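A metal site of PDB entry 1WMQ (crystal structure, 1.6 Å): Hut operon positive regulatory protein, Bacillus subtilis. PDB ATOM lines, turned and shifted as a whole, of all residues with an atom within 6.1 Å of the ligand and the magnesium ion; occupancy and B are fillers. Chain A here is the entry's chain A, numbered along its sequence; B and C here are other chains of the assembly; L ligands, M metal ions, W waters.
Water W1 lies within hydrogen-bond range of the side-chain carboxylate (OE1) of Glu 80 of chain C and the backbone carbonyl oxygen (O) of Ile 144 of chain C.
Water W2 bridges O of Leu 96 and N2 of the ligand.
Ile 128 touches the ligand (CD1 to O2, 3.6 Å).
Gly 129 touches the ligand.
Tyr 75 of chain B touches the ligand.
Within 4 Å of the ligand: Arg 87, Arg 97, Ile 128, Gly 129, Ala 130, His 137, Tyr 68 of chain B, Tyr 75 of chain B and His 76 of chain B.
The nearest printed residue that does not touch the ligand is Leu 96 (4.03 Å).
The backbone NH (N) of Ile 128 lies within hydrogen-bond range of the backbone carbonyl oxygen (O) of His 137, at 2.9 Å.
NH2 of Arg 97 lies within hydrogen-bond range of O of Thr 86 (3.1 Å).
The side-chain carboxylate (OE1) of Glu 80 of chain C lies within salt-bridge range of the guanidinium group (NH1) of Arg 87 (2.9 Å).
The guanidinium group (NH2) of Arg 87 is in hydrogen-bond range of the backbone carbonyl oxygen (O) of Val 85 (2.8 Å).
The backbone NH (N) of Ala 130 sits at hydrogen-bond distance from the backbone carbonyl oxygen (O) of Leu 135 (2.9 Å).
O of Leu 95 lies within hydrogen-bond range of OH of Tyr 75 of chain B (2.6 Å).
The backbone carbonyl oxygen (O) of Gly 129 lies within hydrogen-bond range of the backbone NH (N) of Thr 98, 2.9 Å away.
OH of Tyr 68 of chain B sits at hydrogen-bond distance from N1 of the ligand, 2.7 Å away.
The guanidinium group (NH1) of Arg 97 is in salt-bridge range of an oxygen (O2) of the ligand (2.8 Å).
NH2 of Arg 87 lies within salt-bridge range of O2 of the ligand (2.9 Å).
A nitrogen (N2) of the ligand lies close to the backbone NH of Ala 130 (3.3 Å).
The magnesium ion is bound by O1 of the ligand (2.1 Å), water W1 (2.2 Å), NE2 of His 72 of chain B (2.3 Å), NE2 of His 76 of chain B (2.3 Å) and NE2 of His 137 (2.3 Å).
The magnesium ion has five donor atoms within binding distance.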
ATOM      1  N   VAL A  85      15.237  18.640  17.411  1.00  0.00           N
ATOM      2  CA  VAL A  85      14.941  19.945  16.840  1.00  0.00           C
ATOM      3  C   VAL A  85      14.348  19.862  15.444  1.00  0.00           C
ATOM      4  O   VAL A  85      13.378  20.557  15.151  1.00  0.00           O
ATOM      5  CB  VAL A  85      16.221  20.824  16.805  1.00  0.00           C
ATOM      6  CG1 VAL A  85      15.983  22.079  15.974  1.00  0.00           C
ATOM      7  CG2 VAL A  85      16.606  21.214  18.231  1.00  0.00           C
ATOM      8  N   THR A  86      14.905  18.996  14.591  1.00  0.00           N
ATOM      9  CA  THR A  86      14.450  18.854  13.218  1.00  0.00           C
ATOM     10  C   THR A  86      13.355  17.832  12.962  1.00  0.00           C
ATOM     11  O   THR A  86      12.628  17.924  11.972  1.00  0.00           O
ATOM     12  CB  THR A  86      15.625  18.571  12.266  1.00  0.00           C
ATOM     13  OG1 THR A  86      16.331  17.408  12.706  1.00  0.00           O
ATOM     14  CG2 THR A  86      16.582  19.773  12.251  1.00  0.00           C
ATOM     15  N   ARG A  87      13.257  16.833  13.837  1.00  0.00           N
ATOM     16  CA  ARG A  87      12.229  15.810  13.744  1.00  0.00           C
ATOM     17  C   ARG A  87      11.994  15.111  12.394  1.00  0.00           C
ATOM     18  O   ARG A  87      10.880  15.137  11.855  1.00  0.00           O
ATOM     19  CB  ARG A  87      10.902  16.395  14.261  1.00  0.00           C
ATOM     20  CG  ARG A  87      10.885  16.660  15.764  1.00  0.00           C
ATOM     21  CD  ARG A  87      10.056  17.893  16.117  1.00  0.00           C
ATOM     22  NE  ARG A  87      10.687  19.098  15.557  1.00  0.00           N
ATOM     23  CZ  ARG A  87      10.098  19.930  14.706  1.00  0.00           C
ATOM     24  NH1 ARG A  87       8.855  19.737  14.307  1.00  0.00           N
ATOM     25  NH2 ARG A  87      10.789  20.954  14.215  1.00  0.00           N
ATOM     26  N   LEU A  95      14.620  23.440   3.609  1.00  0.00           N
ATOM     27  CA  LEU A  95      13.208  23.113   3.774  1.00  0.00           C
ATOM     28  C   LEU A  95      12.459  24.366   4.198  1.00  0.00           C
ATOM     29  O   LEU A  95      11.407  24.307   4.841  1.00  0.00           O
ATOM     30  CB  LEU A  95      13.022  22.002   4.822  1.00  0.00           C
ATOM     31  CG  LEU A  95      13.558  20.619   4.461  1.00  0.00           C
ATOM     32  CD1 LEU A  95      13.167  19.640   5.563  1.00  0.00           C
ATOM     33  CD2 LEU A  95      13.000  20.175   3.116  1.00  0.00           C
ATOM     34  N   LEU A  96      13.018  25.510   3.834  1.00  0.00           N
ATOM     35  CA  LEU A  96      12.418  26.803   4.125  1.00  0.00           C
ATOM     36  C   LEU A  96      12.055  27.056   5.593  1.00  0.00           C
ATOM     37  O   LEU A  96      10.956  27.509   5.911  1.00  0.00           O
ATOM     38  CB  LEU A  96      11.205  27.015   3.216  1.00  0.00           C
ATOM     39  CG  LEU A  96      10.761  28.464   2.975  1.00  0.00           C
ATOM     40  CD1 LEU A  96      11.923  29.268   2.404  1.00  0.00           C
ATOM     41  CD2 LEU A  96       9.585  28.471   2.017  1.00  0.00           C
ATOM     42  N   ARG A  97      12.979  26.725   6.483  1.00  0.00           N
ATOM     43  CA  ARG A  97      12.759  26.976   7.900  1.00  0.00           C
ATOM     44  C   ARG A  97      14.035  27.470   8.561  1.00  0.00           C
ATOM     45  O   ARG A  97      15.153  27.224   8.088  1.00  0.00           O
ATOM     46  CB  ARG A  97      12.186  25.738   8.624  1.00  0.00           C
ATOM     47  CG  ARG A  97      13.038  24.505   8.634  1.00  0.00           C
ATOM     48  CD  ARG A  97      12.338  23.380   9.428  1.00  0.00           C
ATOM     49  NE  ARG A  97      13.117  22.154   9.378  1.00  0.00           N
ATOM     50  CZ  ARG A  97      12.748  20.993   9.900  1.00  0.00           C
ATOM     51  NH1 ARG A  97      11.586  20.877  10.539  1.00  0.00           N
ATOM     52  NH2 ARG A  97      13.545  19.939   9.772  1.00  0.00           N
ATOM     53  N   THR A  98      13.846  28.183   9.655  1.00  0.00           N
ATOM     54  CA  THR A  98      14.953  28.786  10.384  1.00  0.00           C
ATOM     55  C   THR A  98      14.822  28.453  11.857  1.00  0.00           C
ATOM     56  O   THR A  98      13.715  28.183  12.345  1.00  0.00           O
ATOM     57  CB  THR A  98      14.900  30.325  10.204  1.00  0.00           C
ATOM     58  OG1 THR A  98      15.871  30.949  11.056  1.00  0.00           O
ATOM     59  CG2 THR A  98      13.511  30.860  10.560  1.00  0.00           C
ATOM     60  N   ILE A 128      11.543  27.331  15.908  1.00  0.00           N
ATOM     61  CA  ILE A 128      11.811  26.907  14.541  1.00  0.00           C
ATOM     62  C   ILE A 128      10.562  27.361  13.784  1.00  0.00           C
ATOM     63  O   ILE A 128       9.459  27.307  14.312  1.00  0.00           O
ATOM     64  CB  ILE A 128      12.010  25.361  14.465  1.00  0.00           C
ATOM     65  CG1 ILE A 128      12.462  24.952  13.068  1.00  0.00           C
ATOM     66  CG2 ILE A 128      10.729  24.641  14.886  1.00  0.00           C
ATOM     67  CD1 ILE A 128      12.916  23.492  12.957  1.00  0.00           C
ATOM     68  N   GLY A 129      10.738  27.849  12.564  1.00  0.00           N
ATOM     69  CA  GLY A 129       9.575  28.294  11.828  1.00  0.00           C
ATOM     70  C   GLY A 129       9.913  28.761  10.441  1.00  0.00           C
ATOM     71  O   GLY A 129      11.020  28.555   9.961  1.00  0.00           O
ATOM     72  N   ALA A 130       8.945  29.381   9.784  1.00  0.00           N
ATOM     73  CA  ALA A 130       9.148  29.914   8.461  1.00  0.00           C
ATOM     74  C   ALA A 130      10.023  31.141   8.678  1.00  0.00           C
ATOM     75  O   ALA A 130      10.087  31.677   9.777  1.00  0.00           O
ATOM     76  CB  ALA A 130       7.827  30.314   7.841  1.00  0.00           C
ATOM     77  N   PRO A 131      10.715  31.600   7.633  1.00  0.00           N
ATOM     78  CA  PRO A 131      11.584  32.771   7.733  1.00  0.00           C
ATOM     79  C   PRO A 131      10.734  34.036   7.837  1.00  0.00           C
ATOM     80  O   PRO A 131      10.774  34.906   6.967  1.00  0.00           O
ATOM     81  CB  PRO A 131      12.386  32.733   6.427  1.00  0.00           C
ATOM     82  CG  PRO A 131      12.149  31.351   5.868  1.00  0.00           C
ATOM     83  CD  PRO A 131      10.741  31.051   6.261  1.00  0.00           C
ATOM     84  N   LEU A 135       5.931  33.446  12.758  1.00  0.00           N
ATOM     85  CA  LEU A 135       5.454  32.195  12.167  1.00  0.00           C
ATOM     86  C   LEU A 135       6.405  31.101  12.625  1.00  0.00           C
ATOM     87  O   LEU A 135       7.213  30.576  11.847  1.00  0.00           O
ATOM     88  CB  LEU A 135       5.435  32.297  10.645  1.00  0.00           C
ATOM     89  CG  LEU A 135       4.617  33.447  10.044  1.00  0.00           C
ATOM     90  CD1 LEU A 135       4.569  33.311   8.534  1.00  0.00           C
ATOM     91  CD2 LEU A 135       3.207  33.432  10.607  1.00  0.00           C
ATOM     92  N   GLU A 136       6.297  30.754  13.899  1.00  0.00           N
ATOM     93  CA  GLU A 136       7.188  29.785  14.518  1.00  0.00           C
ATOM     94  C   GLU A 136       6.590  29.176  15.778  1.00  0.00           C
ATOM     95  O   GLU A 136       5.606  29.681  16.312  1.00  0.00           O
ATOM     96  CB  GLU A 136       8.480  30.507  14.916  1.00  0.00           C
ATOM     97  CG  GLU A 136       8.199  31.604  15.967  1.00  0.00           C
ATOM     98  CD  GLU A 136       9.249  32.706  15.995  1.00  0.00           C
ATOM     99  OE1 GLU A 136       9.598  33.199  14.912  1.00  0.00           O
ATOM    100  OE2 GLU A 136       9.696  33.076  17.104  1.00  0.00           O
ATOM    101  N   HIS A 137       7.198  28.083  16.230  1.00  0.00           N
ATOM    102  CA  HIS A 137       6.817  27.456  17.478  1.00  0.00           C
ATOM    103  C   HIS A 137       8.100  26.945  18.134  1.00  0.00           C
ATOM    104  O   HIS A 137       9.168  26.961  17.519  1.00  0.00           O
ATOM    105  CB  HIS A 137       5.758  26.343  17.299  1.00  0.00           C
ATOM    106  CG  HIS A 137       6.183  25.178  16.452  1.00  0.00           C
ATOM    107  ND1 HIS A 137       7.205  24.330  16.810  1.00  0.00           N
ATOM    108  CD2 HIS A 137       5.659  24.683  15.310  1.00  0.00           C
ATOM    109  CE1 HIS A 137       7.288  23.347  15.929  1.00  0.00           C
ATOM    110  NE2 HIS A 137       6.356  23.545  15.012  1.00  0.00           N
ATOM    111  N   TYR B  68      -0.235  32.138  12.013  1.00  0.00           N
ATOM    112  CA  TYR B  68       0.653  31.001  11.788  1.00  0.00           C
ATOM    113  C   TYR B  68      -0.109  29.704  11.619  1.00  0.00           C
ATOM    114  O   TYR B  68       0.235  28.880  10.780  1.00  0.00           O
ATOM    115  CB  TYR B  68       1.626  30.875  12.960  1.00  0.00           C
ATOM    116  CG  TYR B  68       2.656  29.776  12.809  1.00  0.00           C
ATOM    117  CD1 TYR B  68       3.366  29.602  11.627  1.00  0.00           C
ATOM    118  CD2 TYR B  68       2.972  28.955  13.891  1.00  0.00           C
ATOM    119  CE1 TYR B  68       4.375  28.644  11.513  1.00  0.00           C
ATOM    120  CE2 TYR B  68       3.985  27.994  13.799  1.00  0.00           C
ATOM    121  CZ  TYR B  68       4.682  27.844  12.604  1.00  0.00           C
ATOM    122  OH  TYR B  68       5.695  26.915  12.526  1.00  0.00           O
ATOM    123  N   SER B  71      -0.690  28.360   8.186  1.00  0.00           N
ATOM    124  CA  SER B  71       0.572  28.189   7.469  1.00  0.00           C
ATOM    125  C   SER B  71       1.263  26.957   8.025  1.00  0.00           C
ATOM    126  O   SER B  71       1.924  26.200   7.298  1.00  0.00           O
ATOM    127  CB  SER B  71       1.477  29.403   7.643  1.00  0.00           C
ATOM    128  OG  SER B  71       0.942  30.531   6.968  1.00  0.00           O
ATOM    129  N   HIS B  72       1.111  26.734   9.329  1.00  0.00           N
ATOM    130  CA  HIS B  72       1.719  25.580   9.979  1.00  0.00           C
ATOM    131  C   HIS B  72       1.111  24.308   9.407  1.00  0.00           C
ATOM    132  O   HIS B  72       1.813  23.349   9.102  1.00  0.00           O
ATOM    133  CB  HIS B  72       1.514  25.642  11.498  1.00  0.00           C
ATOM    134  CG  HIS B  72       2.190  24.536  12.240  1.00  0.00           C
ATOM    135  ND1 HIS B  72       1.520  23.425  12.701  1.00  0.00           N
ATOM    136  CD2 HIS B  72       3.479  24.364  12.596  1.00  0.00           C
ATOM    137  CE1 HIS B  72       2.366  22.619  13.306  1.00  0.00           C
ATOM    138  NE2 HIS B  72       3.564  23.167  13.264  1.00  0.00           N
ATOM    139  N   TYR B  75       2.387  23.785   5.823  1.00  0.00           N
ATOM    140  CA  TYR B  75       3.792  23.389   5.783  1.00  0.00           C
ATOM    141  C   TYR B  75       3.942  21.892   5.998  1.00  0.00           C
ATOM    142  O   TYR B  75       4.636  21.217   5.246  1.00  0.00           O
ATOM    143  CB  TYR B  75       4.599  24.118   6.870  1.00  0.00           C
ATOM    144  CG  TYR B  75       6.062  23.781   6.810  1.00  0.00           C
ATOM    145  CD1 TYR B  75       6.887  24.359   5.842  1.00  0.00           C
ATOM    146  CD2 TYR B  75       6.642  22.878   7.708  1.00  0.00           C
ATOM    147  CE1 TYR B  75       8.244  24.055   5.764  1.00  0.00           C
ATOM    148  CE2 TYR B  75       7.990  22.558   7.638  1.00  0.00           C
ATOM    149  CZ  TYR B  75       8.791  23.152   6.676  1.00  0.00           C
ATOM    150  OH  TYR B  75      10.147  22.879   6.612  1.00  0.00           O
ATOM    151  N   HIS B  76       3.275  21.386   7.023  1.00  0.00           N
ATOM    152  CA  HIS B  76       3.375  19.967   7.318  1.00  0.00           C
ATOM    153  C   HIS B  76       2.710  19.101   6.274  1.00  0.00           C
ATOM    154  O   HIS B  76       3.166  17.992   6.007  1.00  0.00           O
ATOM    155  CB  HIS B  76       2.833  19.693   8.708  1.00  0.00           C
ATOM    156  CG  HIS B  76       3.791  20.071   9.792  1.00  0.00           C
ATOM    157  ND1 HIS B  76       4.874  19.290  10.126  1.00  0.00           N
ATOM    158  CD2 HIS B  76       3.873  21.184  10.563  1.00  0.00           C
ATOM    159  CE1 HIS B  76       5.574  19.891  11.071  1.00  0.00           C
ATOM    160  NE2 HIS B  76       4.990  21.045  11.347  1.00  0.00           N
ATOM    161  N   GLU C  80       6.276  13.550  16.738  1.00  0.00           N
ATOM    162  CA  GLU C  80       7.383  14.503  16.794  1.00  0.00           C
ATOM    163  C   GLU C  80       8.177  14.392  18.086  1.00  0.00           C
ATOM    164  O   GLU C  80       9.403  14.483  18.069  1.00  0.00           O
ATOM    165  CB  GLU C  80       6.862  15.928  16.549  1.00  0.00           C
ATOM    166  CG  GLU C  80       6.450  16.120  15.075  1.00  0.00           C
ATOM    167  CD  GLU C  80       6.168  17.559  14.686  1.00  0.00           C
ATOM    168  OE1 GLU C  80       6.544  18.475  15.438  1.00  0.00           O
ATOM    169  OE2 GLU C  80       5.582  17.777  13.598  1.00  0.00           O
ATOM    170  N   TRP C 119      -3.112  24.972  20.699  1.00  0.00           N
ATOM    171  CA  TRP C 119      -1.994  24.180  20.219  1.00  0.00           C
ATOM    172  C   TRP C 119      -1.760  23.129  21.277  1.00  0.00           C
ATOM    173  O   TRP C 119      -2.244  23.243  22.398  1.00  0.00           O
ATOM    174  CB  TRP C 119      -0.745  25.052  20.042  1.00  0.00           C
ATOM    175  CG  TRP C 119      -0.847  25.977  18.869  1.00  0.00           C
ATOM    176  CD1 TRP C 119      -1.762  26.974  18.693  1.00  0.00           C
ATOM    177  CD2 TRP C 119      -0.051  25.940  17.679  1.00  0.00           C
ATOM    178  NE1 TRP C 119      -1.581  27.566  17.465  1.00  0.00           N
ATOM    179  CE2 TRP C 119      -0.546  26.957  16.825  1.00  0.00           C
ATOM    180  CE3 TRP C 119       1.025  25.152  17.262  1.00  0.00           C
ATOM    181  CZ2 TRP C 119       0.006  27.194  15.565  1.00  0.00           C
ATOM    182  CZ3 TRP C 119       1.569  25.394  16.004  1.00  0.00           C
ATOM    183  CH2 TRP C 119       1.065  26.405  15.178  1.00  0.00           C
ATOM    184  N   ILE C 144       5.182  19.588  19.054  1.00  0.00           N
ATOM    185  CA  ILE C 144       4.193  20.655  19.162  1.00  0.00           C
ATOM    186  C   ILE C 144       3.333  20.690  17.897  1.00  0.00           C
ATOM    187  O   ILE C 144       3.841  20.549  16.796  1.00  0.00           O
ATOM    188  CB  ILE C 144       4.906  22.017  19.358  1.00  0.00           C
ATOM    189  CG1 ILE C 144       5.511  22.091  20.773  1.00  0.00           C
ATOM    190  CG2 ILE C 144       3.910  23.174  19.173  1.00  0.00           C
ATOM    191  CD1 ILE C 144       6.439  23.261  21.006  1.00  0.00           C
ATOM    192  N   ASN C 145       2.023  20.858  18.071  1.00  0.00           N
ATOM    193  CA  ASN C 145       1.120  20.874  16.921  1.00  0.00           C
ATOM    194  C   ASN C 145      -0.092  21.762  17.179  1.00  0.00           C
ATOM    195  O   ASN C 145      -0.422  22.046  18.330  1.00  0.00           O
ATOM    196  CB  ASN C 145       0.662  19.441  16.621  1.00  0.00           C
ATOM    197  CG  ASN C 145       0.233  19.258  15.169  1.00  0.00           C
ATOM    198  OD1 ASN C 145       0.485  20.111  14.311  1.00  0.00           O
ATOM    199  ND2 ASN C 145      -0.384  18.115  14.892  1.00  0.00           N
HETATM  200  C1  LIG L   1       7.762  23.538  11.069  1.00  0.00           C
HETATM  201  C2  LIG L   1       8.443  22.562  12.021  1.00  0.00           C
HETATM  202  O1  LIG L   1       7.751  21.918  12.824  1.00  0.00           O
HETATM  203  C3  LIG L   1       8.562  24.827  10.941  1.00  0.00           C
HETATM  204  C4  LIG L   1       8.008  25.765   9.921  1.00  0.00           C
HETATM  205  N1  LIG L   1       6.846  26.472  10.116  1.00  0.00           N
HETATM  206  C5  LIG L   1       8.405  26.028   8.654  1.00  0.00           C
HETATM  207  C6  LIG L   1       6.543  27.131   9.017  1.00  0.00           C
HETATM  208  N2  LIG L   1       7.472  26.884   8.108  1.00  0.00           N
HETATM  209  O2  LIG L   1       9.673  22.421  11.942  1.00  0.00           O
HETATM  210 MG    MG M   1       5.696  22.302  13.156  1.00  0.00          MG
HETATM  211  O   HOH W   1       5.252  20.601  14.483  1.00  0.00           O
HETATM  212  O   HOH W   2       8.311  28.001   5.639  1.00  0.00           O
